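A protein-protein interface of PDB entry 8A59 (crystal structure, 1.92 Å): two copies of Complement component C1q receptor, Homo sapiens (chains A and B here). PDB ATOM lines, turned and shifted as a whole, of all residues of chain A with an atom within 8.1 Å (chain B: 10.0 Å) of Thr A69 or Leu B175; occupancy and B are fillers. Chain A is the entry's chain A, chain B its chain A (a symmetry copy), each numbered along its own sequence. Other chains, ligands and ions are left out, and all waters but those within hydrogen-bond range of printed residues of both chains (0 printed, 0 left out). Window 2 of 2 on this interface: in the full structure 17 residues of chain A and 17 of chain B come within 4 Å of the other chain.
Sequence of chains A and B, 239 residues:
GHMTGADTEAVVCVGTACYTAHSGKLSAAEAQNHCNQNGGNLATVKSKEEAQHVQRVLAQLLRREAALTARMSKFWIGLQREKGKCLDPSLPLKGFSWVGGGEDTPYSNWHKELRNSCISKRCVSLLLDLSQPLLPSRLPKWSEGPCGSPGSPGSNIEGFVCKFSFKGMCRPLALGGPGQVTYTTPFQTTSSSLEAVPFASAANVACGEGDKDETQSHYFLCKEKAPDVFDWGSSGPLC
The side-chain hydroxyl of Thr A69 is in hydrogen-bond range of the backbone carbonyl oxygen of Gly B179 (3.3 Å).
The backbone NH (N) of Gln B180 lies within hydrogen-bond range of the backbone carbonyl oxygen (O) of Ala B206 (3.0 Å). The side-chain sulfur of Cys B239 forms a disulfide with the side-chain sulfur of Cys B207, at 2.0 Å. O of Ala A67 lies within hydrogen-bond range of OG1 of Thr A69 (3.4 Å).
Among the printed residues, merely in contact across the chains: Leu A62 with Ser B193, Ala A66 with Gly B179, Ala A66 with Gln B180, Ala A66 with Val B181, Ala A67 with Gly B179 and Thr A69 with Leu B175.
Of the printed residues of chain B, Thr A69 touches Leu B175 (3.8 Å) and Gly B179 (3.3 Å). Of chain A, only Thr A69 (3.8 Å) comes within 4 Å of Leu B175. Ala A70 touches none of the printed residues of chain B. Gly B179 touches just these residues of chain A: Ala A66, Ala A67 and Thr A69. Of the printed residues of chain A, Ser B193 touches Leu A62 (3.9 Å). Printed residues of chain B within 4 Å of Ala A67: Gly B179. Of the printed residues of chain B, Ala A66 touches Gly B179, Gln B180 and Val B181. Of the printed residues of chain B, Leu A62 touches Ser B193. Printed residues of chain A within 4 Å of Gln B180: Ala A66 (3.5 Å). The nearest residue of chain B that does not touch Thr A69 is Val B181 (4.6 Å). The nearest residue of chain A that does not touch Leu B175 is Ala A66 (6.2 Å). The nearest printed residue of chain B that does not touch Leu A62 is Ser B192 (4.4 Å).
Hydrophobic or aromatic side chains of chain B that line the printed part of chain A: Leu B175. Along chain A the printed residues that touch a printed residue of chain B span positions 62 to 69. Among the printed residues, 7 pairs touch across the chains. Among the printed residues, no Asp or Glu carboxylate lies within 4 Å of a Lys or Arg side-chain nitrogen of the other chain.
No position is printed for both chains. Of the 7 pairs that touch across the chains among the printed residues, none has its exchanged pair printed and touching as well.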
ATOM      1  N   LEU A  62      33.784 -27.208 -29.775  1.00  0.00           N
ATOM      2  CA  LEU A  62      32.419 -27.206 -29.252  1.00  0.00           C
ATOM      3  C   LEU A  62      31.751 -28.580 -29.359  1.00  0.00           C
ATOM      4  O   LEU A  62      30.987 -28.944 -28.476  1.00  0.00           O
ATOM      5  CB  LEU A  62      31.586 -26.137 -29.946  1.00  0.00           C
ATOM      6  CG  LEU A  62      32.122 -24.728 -29.758  1.00  0.00           C
ATOM      7  CD1 LEU A  62      31.427 -23.764 -30.695  1.00  0.00           C
ATOM      8  CD2 LEU A  62      32.042 -24.300 -28.304  1.00  0.00           C
ATOM      9  N   GLU A  65      33.636 -30.790 -26.498  1.00  0.00           N
ATOM     10  CA  GLU A  65      33.518 -30.424 -25.087  1.00  0.00           C
ATOM     11  C   GLU A  65      32.091 -29.977 -24.761  1.00  0.00           C
ATOM     12  O   GLU A  65      31.739 -28.805 -24.932  1.00  0.00           O
ATOM     13  CB  GLU A  65      34.540 -29.363 -24.672  1.00  0.00           C
ATOM     14  CG  GLU A  65      35.925 -29.937 -24.424  1.00  0.00           C
ATOM     15  N   ALA A  66      31.294 -30.921 -24.236  1.00  0.00           N
ATOM     16  CA  ALA A  66      29.871 -30.711 -23.968  1.00  0.00           C
ATOM     17  C   ALA A  66      29.663 -29.661 -22.869  1.00  0.00           C
ATOM     18  O   ALA A  66      28.570 -29.105 -22.737  1.00  0.00           O
ATOM     19  CB  ALA A  66      29.188 -32.034 -23.638  1.00  0.00           C
ATOM     20  N   ALA A  67      30.721 -29.409 -22.080  1.00  0.00           N
ATOM     21  CA  ALA A  67      30.724 -28.457 -20.976  1.00  0.00           C
ATOM     22  C   ALA A  67      30.729 -26.998 -21.456  1.00  0.00           C
ATOM     23  O   ALA A  67      30.472 -26.088 -20.667  1.00  0.00           O
ATOM     24  CB  ALA A  67      31.892 -28.763 -20.058  1.00  0.00           C
ATOM     25  N   LEU A  68      31.012 -26.756 -22.744  1.00  0.00           N
ATOM     26  CA  LEU A  68      31.022 -25.395 -23.268  1.00  0.00           C
ATOM     27  C   LEU A  68      29.599 -24.973 -23.623  1.00  0.00           C
ATOM     28  O   LEU A  68      29.076 -25.310 -24.688  1.00  0.00           O
ATOM     29  CB  LEU A  68      31.934 -25.323 -24.495  1.00  0.00           C
ATOM     30  CG  LEU A  68      33.412 -25.095 -24.201  1.00  0.00           C
ATOM     31  CD1 LEU A  68      34.228 -25.355 -25.454  1.00  0.00           C
ATOM     32  CD2 LEU A  68      33.650 -23.677 -23.686  1.00  0.00           C
ATOM     33  N   THR A  69      28.983 -24.221 -22.707  1.00  0.00           N
ATOM     34  CA  THR A  69      27.563 -23.923 -22.814  1.00  0.00           C
ATOM     35  C   THR A  69      27.311 -22.445 -22.501  1.00  0.00           C
ATOM     36  O   THR A  69      26.173 -21.995 -22.565  1.00  0.00           O
ATOM     37  CB  THR A  69      26.746 -24.876 -21.929  1.00  0.00           C
ATOM     38  OG1 THR A  69      27.323 -24.790 -20.628  1.00  0.00           O
ATOM     39  CG2 THR A  69      26.768 -26.318 -22.396  1.00  0.00           C
ATOM     40  N   ALA A  70      28.373 -21.700 -22.147  1.00  0.00           N
ATOM     41  CA  ALA A  70      28.239 -20.297 -21.788  1.00  0.00           C
ATOM     42  C   ALA A  70      27.820 -19.503 -23.023  1.00  0.00           C
ATOM     43  O   ALA A  70      28.492 -19.550 -24.055  1.00  0.00           O
ATOM     44  CB  ALA A  70      29.523 -19.764 -21.196  1.00  0.00           C
ATOM     45  N   ARG A  71      26.715 -18.761 -22.891  1.00  0.00           N
ATOM     46  CA  ARG A  71      26.064 -18.116 -24.022  1.00  0.00           C
ATOM     47  C   ARG A  71      27.082 -17.346 -24.872  1.00  0.00           C
ATOM     48  O   ARG A  71      27.182 -17.580 -26.082  1.00  0.00           O
ATOM     49  CB  ARG A  71      24.926 -17.234 -23.500  1.00  0.00           C
ATOM     50  CG  ARG A  71      24.458 -16.165 -24.472  1.00  0.00           C
ATOM     51  CD  ARG A  71      23.722 -16.777 -25.646  1.00  0.00           C
ATOM     52  NE  ARG A  71      23.239 -15.739 -26.538  1.00  0.00           N
ATOM     53  N   MET A  72      27.803 -16.409 -24.232  1.00  0.00           N
ATOM     54  CA  MET A  72      28.815 -15.584 -24.887  1.00  0.00           C
ATOM     55  C   MET A  72      30.210 -16.078 -24.504  1.00  0.00           C
ATOM     56  O   MET A  72      30.616 -15.977 -23.343  1.00  0.00           O
ATOM     57  CB  MET A  72      28.689 -14.115 -24.471  1.00  0.00           C
ATOM     58  CG  MET A  72      27.431 -13.411 -24.961  1.00  0.00           C
ATOM     59  SD  MET A  72      27.108 -13.601 -26.726  1.00  0.00           S
ATOM     60  CE  MET A  72      26.946 -11.888 -27.226  1.00  0.00           C
ATOM     61  N   SER A  73      30.939 -16.604 -25.497  1.00  0.00           N
ATOM     62  CA  SER A  73      32.166 -17.342 -25.249  1.00  0.00           C
ATOM     63  C   SER A  73      33.319 -16.707 -26.034  1.00  0.00           C
ATOM     64  O   SER A  73      33.228 -16.537 -27.246  1.00  0.00           O
ATOM     65  CB  SER A  73      31.977 -18.776 -25.656  1.00  0.00           C
ATOM     66  OG  SER A  73      31.345 -19.515 -24.626  1.00  0.00           O
ATOM     67  N   LEU A 130      27.003 -18.706 -28.601  1.00  0.00           N
ATOM     68  CA  LEU A 130      26.696 -20.118 -28.707  1.00  0.00           C
ATOM     69  C   LEU A 130      25.188 -20.351 -28.785  1.00  0.00           C
ATOM     70  O   LEU A 130      24.759 -21.497 -28.732  1.00  0.00           O
ATOM     71  CB  LEU A 130      27.293 -20.843 -27.502  1.00  0.00           C
ATOM     72  CG  LEU A 130      28.819 -20.800 -27.444  1.00  0.00           C
ATOM     73  CD1 LEU A 130      29.316 -21.700 -26.334  1.00  0.00           C
ATOM     74  CD2 LEU A 130      29.404 -21.222 -28.785  1.00  0.00           C
ATOM     75  N   SER A 131      24.408 -19.271 -28.938  1.00  0.00           N
ATOM     76  CA  SER A 131      22.990 -19.408 -29.245  1.00  0.00           C
ATOM     77  C   SER A 131      22.714 -19.378 -30.752  1.00  0.00           C
ATOM     78  O   SER A 131      21.589 -19.665 -31.179  1.00  0.00           O
ATOM     79  CB  SER A 131      22.154 -18.397 -28.498  1.00  0.00           C
ATOM     80  OG  SER A 131      22.115 -17.155 -29.194  1.00  0.00           O
ATOM     81  N   GLU A 158      36.676 -18.262 -22.167  1.00  0.00           N
ATOM     82  CA  GLU A 158      36.317 -19.663 -22.042  1.00  0.00           C
ATOM     83  C   GLU A 158      37.443 -20.510 -22.618  1.00  0.00           C
ATOM     84  O   GLU A 158      37.442 -21.732 -22.497  1.00  0.00           O
ATOM     85  CB  GLU A 158      35.038 -19.924 -22.854  1.00  0.00           C
ATOM     86  CG  GLU A 158      33.747 -19.402 -22.224  1.00  0.00           C
ATOM     87  CD  GLU A 158      33.308 -20.001 -20.888  1.00  0.00           C
ATOM     88  OE1 GLU A 158      32.817 -19.234 -20.024  1.00  0.00           O
ATOM     89  OE2 GLU A 158      33.461 -21.227 -20.701  1.00  0.00           O
ATOM     90  N   ARG B 171      15.365 -24.295 -30.286  1.00  0.00           N
ATOM     91  CA  ARG B 171      16.702 -23.736 -30.144  1.00  0.00           C
ATOM     92  C   ARG B 171      17.471 -24.569 -29.116  1.00  0.00           C
ATOM     93  O   ARG B 171      16.870 -25.270 -28.304  1.00  0.00           O
ATOM     94  CB  ARG B 171      16.660 -22.252 -29.781  1.00  0.00           C
ATOM     95  CG  ARG B 171      15.572 -21.464 -30.497  1.00  0.00           C
ATOM     96  CD  ARG B 171      15.835 -20.027 -30.888  1.00  0.00           C
ATOM     97  NE  ARG B 171      15.682 -19.005 -29.854  1.00  0.00           N
ATOM     98  CZ  ARG B 171      14.888 -17.932 -29.929  1.00  0.00           C
ATOM     99  NH1 ARG B 171      14.846 -17.073 -28.924  1.00  0.00           N
ATOM    100  NH2 ARG B 171      14.140 -17.715 -31.000  1.00  0.00           N
ATOM    101  N   PRO B 172      18.821 -24.617 -29.157  1.00  0.00           N
ATOM    102  CA  PRO B 172      19.561 -25.488 -28.232  1.00  0.00           C
ATOM    103  C   PRO B 172      19.255 -25.105 -26.778  1.00  0.00           C
ATOM    104  O   PRO B 172      19.031 -23.934 -26.486  1.00  0.00           O
ATOM    105  CB  PRO B 172      21.032 -25.218 -28.593  1.00  0.00           C
ATOM    106  CG  PRO B 172      20.984 -24.660 -30.023  1.00  0.00           C
ATOM    107  CD  PRO B 172      19.686 -23.881 -30.102  1.00  0.00           C
ATOM    108  N   LEU B 173      19.237 -26.099 -25.885  1.00  0.00           N
ATOM    109  CA  LEU B 173      18.856 -25.921 -24.484  1.00  0.00           C
ATOM    110  C   LEU B 173      19.915 -25.104 -23.737  1.00  0.00           C
ATOM    111  O   LEU B 173      21.057 -25.532 -23.626  1.00  0.00           O
ATOM    112  CB  LEU B 173      18.691 -27.310 -23.850  1.00  0.00           C
ATOM    113  CG  LEU B 173      17.472 -27.505 -22.941  1.00  0.00           C
ATOM    114  CD1 LEU B 173      17.456 -28.907 -22.343  1.00  0.00           C
ATOM    115  CD2 LEU B 173      17.422 -26.449 -21.843  1.00  0.00           C
ATOM    116  N   ALA B 174      19.520 -23.931 -23.225  1.00  0.00           N
ATOM    117  CA  ALA B 174      20.391 -23.044 -22.466  1.00  0.00           C
ATOM    118  C   ALA B 174      20.632 -23.593 -21.057  1.00  0.00           C
ATOM    119  O   ALA B 174      19.845 -24.400 -20.558  1.00  0.00           O
ATOM    120  CB  ALA B 174      19.768 -21.670 -22.402  1.00  0.00           C
ATOM    121  N   LEU B 175      21.726 -23.136 -20.425  1.00  0.00           N
ATOM    122  CA  LEU B 175      22.035 -23.438 -19.032  1.00  0.00           C
ATOM    123  C   LEU B 175      22.184 -22.138 -18.235  1.00  0.00           C
ATOM    124  O   LEU B 175      21.734 -21.103 -18.755  1.00  0.00           O
ATOM    125  CB  LEU B 175      23.321 -24.267 -18.947  1.00  0.00           C
ATOM    126  CG  LEU B 175      23.203 -25.706 -19.445  1.00  0.00           C
ATOM    127  CD1 LEU B 175      24.374 -26.543 -18.959  1.00  0.00           C
ATOM    128  CD2 LEU B 175      21.886 -26.331 -19.004  1.00  0.00           C
ATOM    129  N   PRO B 178      25.617 -23.903 -16.086  1.00  0.00           N
ATOM    130  CA  PRO B 178      26.962 -24.456 -15.816  1.00  0.00           C
ATOM    131  C   PRO B 178      26.959 -25.974 -15.605  1.00  0.00           C
ATOM    132  O   PRO B 178      26.501 -26.452 -14.567  1.00  0.00           O
ATOM    133  CB  PRO B 178      27.385 -23.682 -14.557  1.00  0.00           C
ATOM    134  CG  PRO B 178      26.780 -22.306 -14.772  1.00  0.00           C
ATOM    135  CD  PRO B 178      25.481 -22.550 -15.517  1.00  0.00           C
ATOM    136  N   GLY B 179      27.504 -26.706 -16.595  1.00  0.00           N
ATOM    137  CA  GLY B 179      27.332 -28.144 -16.787  1.00  0.00           C
ATOM    138  C   GLY B 179      27.348 -28.516 -18.276  1.00  0.00           C
ATOM    139  O   GLY B 179      27.769 -27.700 -19.102  1.00  0.00           O
ATOM    140  N   GLN B 180      26.828 -29.714 -18.611  1.00  0.00           N
ATOM    141  CA  GLN B 180      26.908 -30.338 -19.935  1.00  0.00           C
ATOM    142  C   GLN B 180      25.529 -30.769 -20.467  1.00  0.00           C
ATOM    143  O   GLN B 180      24.699 -31.254 -19.697  1.00  0.00           O
ATOM    144  CB  GLN B 180      27.762 -31.600 -19.800  1.00  0.00           C
ATOM    145  N   VAL B 181      25.289 -30.648 -21.795  1.00  0.00           N
ATOM    146  CA  VAL B 181      24.042 -31.099 -22.430  1.00  0.00           C
ATOM    147  C   VAL B 181      24.309 -31.924 -23.695  1.00  0.00           C
ATOM    148  O   VAL B 181      25.230 -31.618 -24.451  1.00  0.00           O
ATOM    149  CB  VAL B 181      23.069 -29.946 -22.762  1.00  0.00           C
ATOM    150  CG1 VAL B 181      21.759 -30.464 -23.354  1.00  0.00           C
ATOM    151  CG2 VAL B 181      22.801 -29.014 -21.588  1.00  0.00           C
ATOM    152  N   THR B 182      23.415 -32.890 -23.964  1.00  0.00           N
ATOM    153  CA  THR B 182      23.545 -33.888 -25.021  1.00  0.00           C
ATOM    154  C   THR B 182      22.177 -34.281 -25.603  1.00  0.00           C
ATOM    155  O   THR B 182      21.433 -35.088 -25.018  1.00  0.00           O
ATOM    156  CB  THR B 182      24.179 -35.169 -24.469  1.00  0.00           C
ATOM    157  N   TYR B 183      21.881 -33.771 -26.813  1.00  0.00           N
ATOM    158  CA  TYR B 183      20.578 -33.976 -27.441  1.00  0.00           C
ATOM    159  C   TYR B 183      20.537 -35.324 -28.158  1.00  0.00           C
ATOM    160  O   TYR B 183      21.528 -35.774 -28.728  1.00  0.00           O
ATOM    161  CB  TYR B 183      20.218 -32.835 -28.400  1.00  0.00           C
ATOM    162  CG  TYR B 183      20.492 -31.448 -27.882  1.00  0.00           C
ATOM    163  CD1 TYR B 183      19.572 -30.770 -27.108  1.00  0.00           C
ATOM    164  CD2 TYR B 183      21.699 -30.827 -28.152  1.00  0.00           C
ATOM    165  CE1 TYR B 183      19.849 -29.493 -26.633  1.00  0.00           C
ATOM    166  CE2 TYR B 183      21.987 -29.550 -27.695  1.00  0.00           C
ATOM    167  CZ  TYR B 183      21.051 -28.881 -26.932  1.00  0.00           C
ATOM    168  OH  TYR B 183      21.358 -27.642 -26.436  1.00  0.00           O
ATOM    169  N   SER B 192      25.890 -33.941 -29.429  1.00  0.00           N
ATOM    170  CA  SER B 192      25.953 -32.655 -28.756  1.00  0.00           C
ATOM    171  C   SER B 192      26.204 -31.553 -29.780  1.00  0.00           C
ATOM    172  O   SER B 192      26.511 -31.824 -30.946  1.00  0.00           O
ATOM    173  CB  SER B 192      27.019 -32.648 -27.681  1.00  0.00           C
ATOM    174  OG  SER B 192      27.417 -31.315 -27.367  1.00  0.00           O
ATOM    175  N   SER B 193      26.050 -30.305 -29.321  1.00  0.00           N
ATOM    176  CA  SER B 193      26.186 -29.134 -30.164  1.00  0.00           C
ATOM    177  C   SER B 193      25.368 -29.296 -31.455  1.00  0.00           C
ATOM    178  O   SER B 193      25.930 -29.364 -32.544  1.00  0.00           O
ATOM    179  CB  SER B 193      27.648 -28.897 -30.434  1.00  0.00           C
ATOM    180  OG  SER B 193      27.894 -27.543 -30.770  1.00  0.00           O
ATOM    181  N   LEU B 194      24.037 -29.416 -31.345  1.00  0.00           N
ATOM    182  CA  LEU B 194      23.167 -29.256 -32.506  1.00  0.00           C
ATOM    183  C   LEU B 194      22.738 -27.805 -32.574  1.00  0.00           C
ATOM    184  O   LEU B 194      22.446 -27.199 -31.547  1.00  0.00           O
ATOM    185  CB  LEU B 194      21.960 -30.183 -32.401  1.00  0.00           C
ATOM    186  CG  LEU B 194      22.287 -31.640 -32.668  1.00  0.00           C
ATOM    187  CD1 LEU B 194      21.077 -32.514 -32.412  1.00  0.00           C
ATOM    188  CD2 LEU B 194      22.824 -31.812 -34.087  1.00  0.00           C
ATOM    189  N   ALA B 203      16.326 -34.356 -24.965  1.00  0.00           N
ATOM    190  CA  ALA B 203      17.624 -33.877 -24.521  1.00  0.00           C
ATOM    191  C   ALA B 203      18.016 -34.609 -23.228  1.00  0.00           C
ATOM    192  O   ALA B 203      17.145 -35.002 -22.449  1.00  0.00           O
ATOM    193  CB  ALA B 203      17.558 -32.411 -24.283  1.00  0.00           C
ATOM    194  N   ASN B 204      19.329 -34.759 -22.988  1.00  0.00           N
ATOM    195  CA  ASN B 204      19.859 -35.377 -21.778  1.00  0.00           C
ATOM    196  C   ASN B 204      20.896 -34.442 -21.143  1.00  0.00           C
ATOM    197  O   ASN B 204      21.984 -34.282 -21.684  1.00  0.00           O
ATOM    198  CB  ASN B 204      20.382 -36.785 -22.085  1.00  0.00           C
ATOM    199  N   VAL B 205      20.531 -33.777 -20.028  1.00  0.00           N
ATOM    200  CA  VAL B 205      21.347 -32.765 -19.363  1.00  0.00           C
ATOM    201  C   VAL B 205      22.076 -33.407 -18.173  1.00  0.00           C
ATOM    202  O   VAL B 205      21.842 -34.577 -17.865  1.00  0.00           O
ATOM    203  CB  VAL B 205      20.506 -31.537 -18.946  1.00  0.00           C
ATOM    204  CG1 VAL B 205      21.328 -30.446 -18.277  1.00  0.00           C
ATOM    205  CG2 VAL B 205      19.692 -30.934 -20.094  1.00  0.00           C
ATOM    206  N   ALA B 206      22.981 -32.641 -17.530  1.00  0.00           N
ATOM    207  CA  ALA B 206      23.805 -33.063 -16.397  1.00  0.00           C
ATOM    208  C   ALA B 206      24.576 -31.858 -15.860  1.00  0.00           C
ATOM    209  O   ALA B 206      25.543 -31.419 -16.485  1.00  0.00           O
ATOM    210  CB  ALA B 206      24.761 -34.152 -16.822  1.00  0.00           C
ATOM    211  N   CYS B 207      24.138 -31.318 -14.711  1.00  0.00           N
ATOM    212  CA  CYS B 207      24.749 -30.114 -14.163  1.00  0.00           C
ATOM    213  C   CYS B 207      26.008 -30.481 -13.363  1.00  0.00           C
ATOM    214  O   CYS B 207      26.797 -29.550 -13.086  1.00  0.00           O
ATOM    215  CB  CYS B 207      23.800 -29.351 -13.244  1.00  0.00           C
ATOM    216  SG  CYS B 207      22.182 -28.957 -13.964  1.00  0.00           S
ATOM    217  N   HIS B 218      18.815 -34.175 -15.864  1.00  0.00           N
ATOM    218  CA  HIS B 218      17.440 -33.864 -16.228  1.00  0.00           C
ATOM    219  C   HIS B 218      17.182 -34.235 -17.692  1.00  0.00           C
ATOM    220  O   HIS B 218      18.078 -34.076 -18.514  1.00  0.00           O
ATOM    221  CB  HIS B 218      17.157 -32.401 -15.849  1.00  0.00           C
ATOM    222  CG  HIS B 218      17.501 -32.079 -14.429  1.00  0.00           C
ATOM    223  ND1 HIS B 218      17.661 -33.064 -13.461  1.00  0.00           N
ATOM    224  CD2 HIS B 218      17.680 -30.897 -13.801  1.00  0.00           C
ATOM    225  CE1 HIS B 218      17.946 -32.499 -12.305  1.00  0.00           C
ATOM    226  NE2 HIS B 218      17.957 -31.170 -12.487  1.00  0.00           N
ATOM    227  N   PHE B 220      14.321 -33.913 -20.958  1.00  0.00           N
ATOM    228  CA  PHE B 220      13.209 -33.147 -21.501  1.00  0.00           C
ATOM    229  C   PHE B 220      12.985 -33.462 -22.977  1.00  0.00           C
ATOM    230  O   PHE B 220      13.909 -33.893 -23.659  1.00  0.00           O
ATOM    231  CB  PHE B 220      13.563 -31.667 -21.521  1.00  0.00           C
ATOM    232  CG  PHE B 220      14.073 -31.111 -20.225  1.00  0.00           C
ATOM    233  CD1 PHE B 220      15.399 -31.273 -19.856  1.00  0.00           C
ATOM    234  CD2 PHE B 220      13.240 -30.364 -19.410  1.00  0.00           C
ATOM    235  CE1 PHE B 220      15.872 -30.720 -18.677  1.00  0.00           C
ATOM    236  CE2 PHE B 220      13.718 -29.808 -18.232  1.00  0.00           C
ATOM    237  CZ  PHE B 220      15.031 -29.991 -17.865  1.00  0.00           C
ATOM    238  N   TRP B 232      11.539 -26.477 -24.845  1.00  0.00           N
ATOM    239  CA  TRP B 232      11.918 -27.609 -24.021  1.00  0.00           C
ATOM    240  C   TRP B 232      10.955 -27.782 -22.840  1.00  0.00           C
ATOM    241  O   TRP B 232      10.872 -28.857 -22.244  1.00  0.00           O
ATOM    242  CB  TRP B 232      13.385 -27.433 -23.589  1.00  0.00           C
ATOM    243  CG  TRP B 232      14.337 -27.660 -24.729  1.00  0.00           C
ATOM    244  CD1 TRP B 232      15.081 -26.717 -25.383  1.00  0.00           C
ATOM    245  CD2 TRP B 232      14.576 -28.907 -25.411  1.00  0.00           C
ATOM    246  NE1 TRP B 232      15.818 -27.305 -26.379  1.00  0.00           N
ATOM    247  CE2 TRP B 232      15.512 -28.643 -26.435  1.00  0.00           C
ATOM    248  CE3 TRP B 232      14.132 -30.223 -25.244  1.00  0.00           C
ATOM    249  CZ2 TRP B 232      15.965 -29.636 -27.290  1.00  0.00           C
ATOM    250  CZ3 TRP B 232      14.587 -31.209 -26.091  1.00  0.00           C
ATOM    251  CH2 TRP B 232      15.500 -30.915 -27.105  1.00  0.00           C
ATOM    252  N   SER B 234      10.831 -25.945 -19.628  1.00  0.00           N
ATOM    253  CA  SER B 234      11.698 -25.967 -18.460  1.00  0.00           C
ATOM    254  C   SER B 234      11.820 -24.549 -17.913  1.00  0.00           C
ATOM    255  O   SER B 234      12.699 -23.799 -18.333  1.00  0.00           O
ATOM    256  CB  SER B 234      13.053 -26.542 -18.802  1.00  0.00           C
ATOM    257  OG  SER B 234      13.692 -25.757 -19.799  1.00  0.00           O
ATOM    258  N   GLY B 236      13.146 -21.935 -15.453  1.00  0.00           N
ATOM    259  CA  GLY B 236      14.391 -21.940 -14.667  1.00  0.00           C
ATOM    260  C   GLY B 236      15.523 -22.553 -15.462  1.00  0.00           C
ATOM    261  O   GLY B 236      15.755 -23.762 -15.304  1.00  0.00           O
ATOM    262  N   PRO B 237      16.220 -21.790 -16.335  1.00  0.00           N
ATOM    263  CA  PRO B 237      17.381 -22.316 -17.030  1.00  0.00           C
ATOM    264  C   PRO B 237      18.057 -23.151 -15.946  1.00  0.00           C
ATOM    265  O   PRO B 237      18.413 -22.597 -14.928  1.00  0.00           O
ATOM    266  CB  PRO B 237      18.138 -21.041 -17.400  1.00  0.00           C
ATOM    267  CG  PRO B 237      17.040 -20.034 -17.653  1.00  0.00           C
ATOM    268  CD  PRO B 237      15.941 -20.394 -16.674  1.00  0.00           C
ATOM    269  N   LEU B 238      18.198 -24.452 -16.181  1.00  0.00           N
ATOM    270  CA  LEU B 238      18.699 -25.329 -15.134  1.00  0.00           C
ATOM    271  C   LEU B 238      20.181 -25.053 -14.879  1.00  0.00           C
ATOM    272  O   LEU B 238      20.814 -24.301 -15.621  1.00  0.00           O
ATOM    273  CB  LEU B 238      18.484 -26.780 -15.578  1.00  0.00           C
ATOM    274  CG  LEU B 238      18.233 -26.973 -17.073  1.00  0.00           C
ATOM    275  CD1 LEU B 238      18.873 -28.251 -17.575  1.00  0.00           C
ATOM    276  CD2 LEU B 238      16.742 -26.964 -17.378  1.00  0.00           C
ATOM    277  N   CYS B 239      20.716 -25.686 -13.822  1.00  0.00           N
ATOM    278  CA  CYS B 239      22.109 -25.593 -13.399  1.00  0.00           C
ATOM    279  C   CYS B 239      22.456 -24.154 -13.003  1.00  0.00           C
ATOM    280  O   CYS B 239      23.571 -23.719 -13.361  1.00  0.00           O
ATOM    281  CB  CYS B 239      23.084 -26.060 -14.477  1.00  0.00           C
ATOM    282  SG  CYS B 239      22.559 -27.536 -15.386  1.00  0.00           S
